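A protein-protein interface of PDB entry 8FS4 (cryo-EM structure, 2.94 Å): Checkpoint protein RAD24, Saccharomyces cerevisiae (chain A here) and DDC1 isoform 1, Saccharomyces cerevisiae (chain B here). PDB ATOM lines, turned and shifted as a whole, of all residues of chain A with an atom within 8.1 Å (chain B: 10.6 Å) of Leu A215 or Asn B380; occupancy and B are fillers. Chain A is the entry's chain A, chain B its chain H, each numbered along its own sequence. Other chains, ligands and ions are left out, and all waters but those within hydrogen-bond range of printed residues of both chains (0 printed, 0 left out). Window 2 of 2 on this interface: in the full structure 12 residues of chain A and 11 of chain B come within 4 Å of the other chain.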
ATOM      1  N   LEU A  97      29.840  23.556 -19.682  1.00  0.00           N
ATOM      2  CA  LEU A  97      30.309  22.713 -20.771  1.00  0.00           C
ATOM      3  C   LEU A  97      30.244  21.245 -20.364  1.00  0.00           C
ATOM      4  O   LEU A  97      30.489  20.918 -19.197  1.00  0.00           O
ATOM      5  CB  LEU A  97      31.745  23.081 -21.148  1.00  0.00           C
ATOM      6  CG  LEU A  97      31.980  24.574 -21.403  1.00  0.00           C
ATOM      7  CD1 LEU A  97      33.452  24.862 -21.659  1.00  0.00           C
ATOM      8  CD2 LEU A  97      31.128  25.076 -22.562  1.00  0.00           C
ATOM      9  N   PRO A  98      29.910  20.340 -21.301  1.00  0.00           N
ATOM     10  CA  PRO A  98      29.716  18.927 -20.941  1.00  0.00           C
ATOM     11  C   PRO A  98      30.739  18.391 -19.952  1.00  0.00           C
ATOM     12  O   PRO A  98      30.368  17.856 -18.902  1.00  0.00           O
ATOM     13  CB  PRO A  98      29.823  18.217 -22.293  1.00  0.00           C
ATOM     14  CG  PRO A  98      29.275  19.209 -23.262  1.00  0.00           C
ATOM     15  CD  PRO A  98      29.608  20.584 -22.723  1.00  0.00           C
ATOM     16  N   ASN A  99      32.023  18.526 -20.271  1.00  0.00           N
ATOM     17  CA  ASN A  99      33.110  18.122 -19.381  1.00  0.00           C
ATOM     18  C   ASN A  99      33.939  19.372 -19.105  1.00  0.00           C
ATOM     19  O   ASN A  99      34.919  19.655 -19.799  1.00  0.00           O
ATOM     20  CB  ASN A  99      33.949  16.999 -19.997  1.00  0.00           C
ATOM     21  CG  ASN A  99      34.658  16.157 -18.952  1.00  0.00           C
ATOM     22  OD1 ASN A  99      35.860  15.911 -19.052  1.00  0.00           O
ATOM     23  ND2 ASN A  99      33.916  15.703 -17.946  1.00  0.00           N
ATOM     24  N   ALA A 100      33.540  20.120 -18.080  1.00  0.00           N
ATOM     25  CA  ALA A 100      34.182  21.380 -17.739  1.00  0.00           C
ATOM     26  C   ALA A 100      35.213  21.140 -16.644  1.00  0.00           C
ATOM     27  O   ALA A 100      34.890  20.576 -15.594  1.00  0.00           O
ATOM     28  CB  ALA A 100      33.143  22.406 -17.290  1.00  0.00           C
ATOM     29  N   ARG A 103      34.462  22.529 -11.611  1.00  0.00           N
ATOM     30  CA  ARG A 103      33.171  22.065 -11.121  1.00  0.00           C
ATOM     31  C   ARG A 103      32.518  23.043 -10.158  1.00  0.00           C
ATOM     32  O   ARG A 103      31.287  23.127 -10.114  1.00  0.00           O
ATOM     33  CB  ARG A 103      33.331  20.713 -10.421  1.00  0.00           C
ATOM     34  CG  ARG A 103      32.900  19.520 -11.256  1.00  0.00           C
ATOM     35  CD  ARG A 103      33.029  18.229 -10.465  1.00  0.00           C
ATOM     36  NE  ARG A 103      32.861  17.045 -11.300  1.00  0.00           N
ATOM     37  CZ  ARG A 103      32.940  15.798 -10.856  1.00  0.00           C
ATOM     38  NH1 ARG A 103      33.192  15.531  -9.585  1.00  0.00           N
ATOM     39  NH2 ARG A 103      32.767  14.794 -11.710  1.00  0.00           N
ATOM     40  N   ARG A 174      22.140  16.822  -7.695  1.00  0.00           N
ATOM     41  CA  ARG A 174      22.959  16.299  -8.776  1.00  0.00           C
ATOM     42  C   ARG A 174      22.140  15.841  -9.969  1.00  0.00           C
ATOM     43  O   ARG A 174      22.680  15.761 -11.076  1.00  0.00           O
ATOM     44  CB  ARG A 174      23.811  15.121  -8.281  1.00  0.00           C
ATOM     45  CG  ARG A 174      24.431  15.329  -6.906  1.00  0.00           C
ATOM     46  CD  ARG A 174      24.419  14.052  -6.086  1.00  0.00           C
ATOM     47  NE  ARG A 174      25.408  14.090  -5.016  1.00  0.00           N
ATOM     48  CZ  ARG A 174      26.720  14.081  -5.205  1.00  0.00           C
ATOM     49  NH1 ARG A 174      27.244  14.017  -6.418  1.00  0.00           N
ATOM     50  NH2 ARG A 174      27.528  14.138  -4.150  1.00  0.00           N
ATOM     51  N   TYR A 175      20.855  15.544  -9.769  1.00  0.00           N
ATOM     52  CA  TYR A 175      19.970  15.171 -10.860  1.00  0.00           C
ATOM     53  C   TYR A 175      19.616  16.349 -11.754  1.00  0.00           C
ATOM     54  O   TYR A 175      18.965  16.146 -12.784  1.00  0.00           O
ATOM     55  CB  TYR A 175      18.691  14.547 -10.303  1.00  0.00           C
ATOM     56  CG  TYR A 175      18.899  13.176  -9.709  1.00  0.00           C
ATOM     57  CD1 TYR A 175      19.370  13.025  -8.413  1.00  0.00           C
ATOM     58  CD2 TYR A 175      18.625  12.031 -10.443  1.00  0.00           C
ATOM     59  CE1 TYR A 175      19.563  11.773  -7.864  1.00  0.00           C
ATOM     60  CE2 TYR A 175      18.813  10.774  -9.903  1.00  0.00           C
ATOM     61  CZ  TYR A 175      19.284  10.651  -8.614  1.00  0.00           C
ATOM     62  OH  TYR A 175      19.474   9.401  -8.072  1.00  0.00           O
ATOM     63  N   LEU A 176      20.025  17.567 -11.395  1.00  0.00           N
ATOM     64  CA  LEU A 176      19.737  18.726 -12.228  1.00  0.00           C
ATOM     65  C   LEU A 176      20.691  18.756 -13.418  1.00  0.00           C
ATOM     66  O   LEU A 176      21.363  19.760 -13.673  1.00  0.00           O
ATOM     67  CB  LEU A 176      19.838  20.014 -11.411  1.00  0.00           C
ATOM     68  CG  LEU A 176      18.929  20.080 -10.180  1.00  0.00           C
ATOM     69  CD1 LEU A 176      19.098  21.411  -9.469  1.00  0.00           C
ATOM     70  CD2 LEU A 176      17.467  19.855 -10.554  1.00  0.00           C
ATOM     71  N   VAL A 177      20.740  17.641 -14.147  1.00  0.00           N
ATOM     72  CA  VAL A 177      21.555  17.450 -15.340  1.00  0.00           C
ATOM     73  C   VAL A 177      20.806  17.991 -16.544  1.00  0.00           C
ATOM     74  O   VAL A 177      19.682  18.489 -16.416  1.00  0.00           O
ATOM     75  CB  VAL A 177      21.921  15.967 -15.529  1.00  0.00           C
ATOM     76  CG1 VAL A 177      22.394  15.368 -14.211  1.00  0.00           C
ATOM     77  CG2 VAL A 177      20.741  15.192 -16.072  1.00  0.00           C
ATOM     78  N   MET A 178      21.450  17.937 -17.707  1.00  0.00           N
ATOM     79  CA  MET A 178      20.878  18.429 -18.956  1.00  0.00           C
ATOM     80  C   MET A 178      19.370  18.221 -18.965  1.00  0.00           C
ATOM     81  O   MET A 178      18.875  17.129 -18.666  1.00  0.00           O
ATOM     82  CB  MET A 178      21.513  17.661 -20.126  1.00  0.00           C
ATOM     83  CG  MET A 178      20.882  17.783 -21.538  1.00  0.00           C
ATOM     84  SD  MET A 178      20.278  19.404 -22.090  1.00  0.00           S
ATOM     85  CE  MET A 178      18.527  19.139 -22.156  1.00  0.00           C
ATOM     86  N   SER A 179      18.650  19.280 -19.320  1.00  0.00           N
ATOM     87  CA  SER A 179      17.186  19.363 -19.291  1.00  0.00           C
ATOM     88  C   SER A 179      16.718  19.676 -17.878  1.00  0.00           C
ATOM     89  O   SER A 179      15.534  19.954 -17.646  1.00  0.00           O
ATOM     90  CB  SER A 179      16.514  18.067 -19.774  1.00  0.00           C
ATOM     91  OG  SER A 179      16.237  17.197 -18.692  1.00  0.00           O
ATOM     92  N   TRP A 208      31.677  16.006  -3.596  1.00  0.00           N
ATOM     93  CA  TRP A 208      31.207  16.627  -4.829  1.00  0.00           C
ATOM     94  C   TRP A 208      32.366  16.874  -5.787  1.00  0.00           C
ATOM     95  O   TRP A 208      32.250  16.627  -6.993  1.00  0.00           O
ATOM     96  CB  TRP A 208      30.489  17.938  -4.511  1.00  0.00           C
ATOM     97  CG  TRP A 208      29.902  18.619  -5.707  1.00  0.00           C
ATOM     98  CD1 TRP A 208      30.551  19.426  -6.593  1.00  0.00           C
ATOM     99  CD2 TRP A 208      28.540  18.557  -6.144  1.00  0.00           C
ATOM    100  NE1 TRP A 208      29.680  19.868  -7.558  1.00  0.00           N
ATOM    101  CE2 TRP A 208      28.438  19.348  -7.304  1.00  0.00           C
ATOM    102  CE3 TRP A 208      27.399  17.908  -5.668  1.00  0.00           C
ATOM    103  CZ2 TRP A 208      27.241  19.507  -7.995  1.00  0.00           C
ATOM    104  CZ3 TRP A 208      26.213  18.068  -6.354  1.00  0.00           C
ATOM    105  CH2 TRP A 208      26.142  18.860  -7.505  1.00  0.00           C
ATOM    106  N   SER A 211      33.592  13.530  -7.249  1.00  0.00           N
ATOM    107  CA  SER A 211      32.545  12.659  -7.760  1.00  0.00           C
ATOM    108  C   SER A 211      32.952  12.070  -9.105  1.00  0.00           C
ATOM    109  O   SER A 211      33.533  12.755  -9.953  1.00  0.00           O
ATOM    110  CB  SER A 211      31.231  13.426  -7.902  1.00  0.00           C
ATOM    111  OG  SER A 211      30.345  12.760  -8.785  1.00  0.00           O
ATOM    112  N   SER A 212      32.642  10.790  -9.296  1.00  0.00           N
ATOM    113  CA  SER A 212      32.953  10.081 -10.529  1.00  0.00           C
ATOM    114  C   SER A 212      31.815  10.132 -11.540  1.00  0.00           C
ATOM    115  O   SER A 212      31.929   9.525 -12.609  1.00  0.00           O
ATOM    116  CB  SER A 212      33.304   8.623 -10.222  1.00  0.00           C
ATOM    117  OG  SER A 212      32.162   7.790 -10.323  1.00  0.00           O
ATOM    118  N   GLU A 213      30.729  10.833 -11.231  1.00  0.00           N
ATOM    119  CA  GLU A 213      29.638  10.955 -12.183  1.00  0.00           C
ATOM    120  C   GLU A 213      30.135  11.674 -13.436  1.00  0.00           C
ATOM    121  O   GLU A 213      30.939  12.609 -13.335  1.00  0.00           O
ATOM    122  CB  GLU A 213      28.469  11.721 -11.562  1.00  0.00           C
ATOM    123  CG  GLU A 213      27.092  11.180 -11.914  1.00  0.00           C
ATOM    124  CD  GLU A 213      26.833   9.809 -11.322  1.00  0.00           C
ATOM    125  OE1 GLU A 213      26.440   9.736 -10.139  1.00  0.00           O
ATOM    126  OE2 GLU A 213      27.017   8.804 -12.041  1.00  0.00           O
ATOM    127  N   PRO A 214      29.686  11.273 -14.631  1.00  0.00           N
ATOM    128  CA  PRO A 214      30.231  11.887 -15.848  1.00  0.00           C
ATOM    129  C   PRO A 214      29.681  13.272 -16.121  1.00  0.00           C
ATOM    130  O   PRO A 214      30.333  14.050 -16.829  1.00  0.00           O
ATOM    131  CB  PRO A 214      29.828  10.897 -16.955  1.00  0.00           C
ATOM    132  CG  PRO A 214      28.948   9.838 -16.275  1.00  0.00           C
ATOM    133  CD  PRO A 214      28.549  10.399 -14.953  1.00  0.00           C
ATOM    134  N   LEU A 215      28.508  13.603 -15.588  1.00  0.00           N
ATOM    135  CA  LEU A 215      27.880  14.898 -15.812  1.00  0.00           C
ATOM    136  C   LEU A 215      27.396  15.440 -14.478  1.00  0.00           C
ATOM    137  O   LEU A 215      26.719  14.730 -13.728  1.00  0.00           O
ATOM    138  CB  LEU A 215      26.712  14.779 -16.798  1.00  0.00           C
ATOM    139  CG  LEU A 215      26.945  13.832 -17.979  1.00  0.00           C
ATOM    140  CD1 LEU A 215      26.325  12.468 -17.709  1.00  0.00           C
ATOM    141  CD2 LEU A 215      26.393  14.430 -19.263  1.00  0.00           C
ATOM    142  N   LEU A 216      27.737  16.686 -14.187  1.00  0.00           N
ATOM    143  CA  LEU A 216      27.386  17.342 -12.938  1.00  0.00           C
ATOM    144  C   LEU A 216      26.826  18.724 -13.226  1.00  0.00           C
ATOM    145  O   LEU A 216      27.093  19.304 -14.283  1.00  0.00           O
ATOM    146  CB  LEU A 216      28.603  17.467 -12.012  1.00  0.00           C
ATOM    147  CG  LEU A 216      28.661  16.460 -10.866  1.00  0.00           C
ATOM    148  CD1 LEU A 216      29.145  15.122 -11.378  1.00  0.00           C
ATOM    149  CD2 LEU A 216      29.558  16.965  -9.751  1.00  0.00           C
ATOM    150  N   PRO A 217      26.042  19.278 -12.307  1.00  0.00           N
ATOM    151  CA  PRO A 217      25.521  20.627 -12.497  1.00  0.00           C
ATOM    152  C   PRO A 217      26.545  21.665 -12.081  1.00  0.00           C
ATOM    153  O   PRO A 217      27.387  21.404 -11.209  1.00  0.00           O
ATOM    154  CB  PRO A 217      24.291  20.656 -11.582  1.00  0.00           C
ATOM    155  CG  PRO A 217      24.653  19.737 -10.466  1.00  0.00           C
ATOM    156  CD  PRO A 217      25.581  18.686 -11.038  1.00  0.00           C
ATOM    157  N   PRO A 218      26.511  22.854 -12.679  1.00  0.00           N
ATOM    158  CA  PRO A 218      27.435  23.915 -12.255  1.00  0.00           C
ATOM    159  C   PRO A 218      27.202  24.325 -10.809  1.00  0.00           C
ATOM    160  O   PRO A 218      26.141  24.858 -10.469  1.00  0.00           O
ATOM    161  CB  PRO A 218      27.133  25.061 -13.228  1.00  0.00           C
ATOM    162  CG  PRO A 218      25.784  24.754 -13.795  1.00  0.00           C
ATOM    163  CD  PRO A 218      25.641  23.276 -13.789  1.00  0.00           C
ATOM    164  N   SER B 321      16.405  -0.642 -16.703  1.00  0.00           N
ATOM    165  CA  SER B 321      17.155  -0.261 -15.513  1.00  0.00           C
ATOM    166  C   SER B 321      16.754   1.147 -15.106  1.00  0.00           C
ATOM    167  O   SER B 321      16.800   2.067 -15.927  1.00  0.00           O
ATOM    168  CB  SER B 321      18.666  -0.333 -15.766  1.00  0.00           C
ATOM    169  OG  SER B 321      19.393   0.107 -14.633  1.00  0.00           O
ATOM    170  N   ILE B 322      16.364   1.310 -13.844  1.00  0.00           N
ATOM    171  CA  ILE B 322      15.931   2.597 -13.312  1.00  0.00           C
ATOM    172  C   ILE B 322      16.525   2.765 -11.920  1.00  0.00           C
ATOM    173  O   ILE B 322      16.497   1.831 -11.111  1.00  0.00           O
ATOM    174  CB  ILE B 322      14.391   2.706 -13.272  1.00  0.00           C
ATOM    175  CG1 ILE B 322      13.845   3.185 -14.624  1.00  0.00           C
ATOM    176  CG2 ILE B 322      13.930   3.632 -12.148  1.00  0.00           C
ATOM    177  CD1 ILE B 322      14.261   4.594 -15.022  1.00  0.00           C
ATOM    178  N   ILE B 323      17.060   3.951 -11.644  1.00  0.00           N
ATOM    179  CA  ILE B 323      17.676   4.275 -10.362  1.00  0.00           C
ATOM    180  C   ILE B 323      17.002   5.524  -9.812  1.00  0.00           C
ATOM    181  O   ILE B 323      16.879   6.531 -10.520  1.00  0.00           O
ATOM    182  CB  ILE B 323      19.195   4.491 -10.500  1.00  0.00           C
ATOM    183  CG1 ILE B 323      19.864   3.221 -11.035  1.00  0.00           C
ATOM    184  CG2 ILE B 323      19.802   4.892  -9.157  1.00  0.00           C
ATOM    185  CD1 ILE B 323      21.325   3.399 -11.404  1.00  0.00           C
ATOM    186  N   HIS B 355      11.840   5.951 -19.362  1.00  0.00           N
ATOM    187  CA  HIS B 355      13.238   6.089 -19.730  1.00  0.00           C
ATOM    188  C   HIS B 355      14.032   6.503 -18.502  1.00  0.00           C
ATOM    189  O   HIS B 355      13.465   7.022 -17.535  1.00  0.00           O
ATOM    190  CB  HIS B 355      13.426   7.125 -20.846  1.00  0.00           C
ATOM    191  CG  HIS B 355      13.047   6.625 -22.206  1.00  0.00           C
ATOM    192  ND1 HIS B 355      12.199   7.318 -23.042  1.00  0.00           N
ATOM    193  CD2 HIS B 355      13.405   5.504 -22.876  1.00  0.00           C
ATOM    194  CE1 HIS B 355      12.048   6.644 -24.168  1.00  0.00           C
ATOM    195  NE2 HIS B 355      12.769   5.540 -24.093  1.00  0.00           N
ATOM    196  N   PRO B 356      15.349   6.282 -18.509  1.00  0.00           N
ATOM    197  CA  PRO B 356      16.163   6.724 -17.367  1.00  0.00           C
ATOM    198  C   PRO B 356      16.017   8.204 -17.062  1.00  0.00           C
ATOM    199  O   PRO B 356      16.051   8.591 -15.887  1.00  0.00           O
ATOM    200  CB  PRO B 356      17.591   6.370 -17.803  1.00  0.00           C
ATOM    201  CG  PRO B 356      17.417   5.230 -18.749  1.00  0.00           C
ATOM    202  CD  PRO B 356      16.136   5.504 -19.482  1.00  0.00           C
ATOM    203  N   GLY B 357      15.856   9.045 -18.081  1.00  0.00           N
ATOM    204  CA  GLY B 357      15.666  10.467 -17.880  1.00  0.00           C
ATOM    205  C   GLY B 357      14.250  10.899 -17.587  1.00  0.00           C
ATOM    206  O   GLY B 357      14.014  12.089 -17.360  1.00  0.00           O
ATOM    207  N   ASP B 358      13.292   9.966 -17.579  1.00  0.00           N
ATOM    208  CA  ASP B 358      11.904  10.314 -17.326  1.00  0.00           C
ATOM    209  C   ASP B 358      11.509   9.949 -15.899  1.00  0.00           C
ATOM    210  O   ASP B 358      12.045   8.998 -15.322  1.00  0.00           O
ATOM    211  CB  ASP B 358      10.978   9.588 -18.307  1.00  0.00           C
ATOM    212  CG  ASP B 358      11.306   9.896 -19.754  1.00  0.00           C
ATOM    213  OD1 ASP B 358      12.469  10.252 -20.038  1.00  0.00           O
ATOM    214  OD2 ASP B 358      10.402   9.778 -20.608  1.00  0.00           O
ATOM    215  N   VAL B 376      12.070  11.586  -9.824  1.00  0.00           N
ATOM    216  CA  VAL B 376      12.957  11.720 -10.972  1.00  0.00           C
ATOM    217  C   VAL B 376      14.025  10.637 -10.918  1.00  0.00           C
ATOM    218  O   VAL B 376      14.357  10.108  -9.851  1.00  0.00           O
ATOM    219  CB  VAL B 376      13.585  13.129 -11.014  1.00  0.00           C
ATOM    220  CG1 VAL B 376      14.320  13.433  -9.717  1.00  0.00           C
ATOM    221  CG2 VAL B 376      14.520  13.269 -12.209  1.00  0.00           C
ATOM    222  N   THR B 377      14.568  10.301 -12.086  1.00  0.00           N
ATOM    223  CA  THR B 377      15.624   9.311 -12.213  1.00  0.00           C
ATOM    224  C   THR B 377      16.786   9.920 -12.983  1.00  0.00           C
ATOM    225  O   THR B 377      16.602  10.829 -13.798  1.00  0.00           O
ATOM    226  CB  THR B 377      15.126   8.049 -12.928  1.00  0.00           C
ATOM    227  OG1 THR B 377      14.500   8.410 -14.166  1.00  0.00           O
ATOM    228  CG2 THR B 377      14.124   7.302 -12.058  1.00  0.00           C
ATOM    229  N   ASP B 378      17.988   9.413 -12.714  1.00  0.00           N
ATOM    230  CA  ASP B 378      19.187   9.925 -13.367  1.00  0.00           C
ATOM    231  C   ASP B 378      19.015   9.919 -14.880  1.00  0.00           C
ATOM    232  O   ASP B 378      18.670   8.896 -15.475  1.00  0.00           O
ATOM    233  CB  ASP B 378      20.399   9.076 -12.974  1.00  0.00           C
ATOM    234  CG  ASP B 378      21.079   9.574 -11.716  1.00  0.00           C
ATOM    235  OD1 ASP B 378      21.372  10.785 -11.634  1.00  0.00           O
ATOM    236  OD2 ASP B 378      21.323   8.754 -10.806  1.00  0.00           O
ATOM    237  N   SER B 379      19.264  11.073 -15.501  1.00  0.00           N
ATOM    238  CA  SER B 379      19.125  11.176 -16.950  1.00  0.00           C
ATOM    239  C   SER B 379      20.237  10.412 -17.659  1.00  0.00           C
ATOM    240  O   SER B 379      19.977   9.470 -18.416  1.00  0.00           O
ATOM    241  CB  SER B 379      19.121  12.645 -17.374  1.00  0.00           C
ATOM    242  OG  SER B 379      18.396  13.441 -16.454  1.00  0.00           O
ATOM    243  N   ASN B 380      21.484  10.803 -17.422  1.00  0.00           N
ATOM    244  CA  ASN B 380      22.626  10.117 -18.015  1.00  0.00           C
ATOM    245  C   ASN B 380      23.769  10.009 -17.013  1.00  0.00           C
ATOM    246  O   ASN B 380      23.767   9.136 -16.146  1.00  0.00           O
ATOM    247  CB  ASN B 380      23.095  10.846 -19.276  1.00  0.00           C
ATOM    248  CG  ASN B 380      23.129  12.351 -19.100  1.00  0.00           C
ATOM    249  OD1 ASN B 380      22.786  12.872 -18.040  1.00  0.00           O
ATOM    250  ND2 ASN B 380      23.549  13.057 -20.144  1.00  0.00           N
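OH of Tyr A175 lies close to OD2 of Asp B378, 3.4 Å away.
The backbone carbonyl oxygen (O) of Pro B356 lies close to the backbone carbonyl oxygen (O) of Asp B378 (2.7 Å).
O of Asp B358 is in hydrogen-bond range of OG1 of Thr B377.
Among the printed residues, merely in contact across the chains: Tyr A175 with Thr B377, Val A177 with Ser B379, Val A177 with Asn B380 and Leu A215 with Asn B380.
Of chain B, only Asn B380 (3.3 Å) comes within 4 Å of Leu A215.
Asn B380 touches two residues of chain A.
Glu A213 touches none of the printed residues of chain B.
No residue of chain B comes within 4 Å of Pro A214.
Printed residues of chain A within 4 Å of Ser B379: Val A177.
Of the printed residues of chain B, Tyr A175 touches Thr B377 (3.8 Å) and Asp B378 (3.1 Å).
Ile B323 touches none of the printed residues of chain A.
Met A178 touches none of the printed residues of chain B.
The nearest residue of chain A that does not touch Asn B380 is Met A178 (5.0 Å).
Hydrophobic or aromatic side chains of chain A that line the printed part of chain B: Tyr A175, Val A177 and Leu A215.
Along chain A the printed residues that touch a printed residue of chain B span positions 175 to 215.
Among the printed residues, no Asp or Glu carboxylate lies within 4 Å of a Lys or Arg side-chain nitrogen of the other chain.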
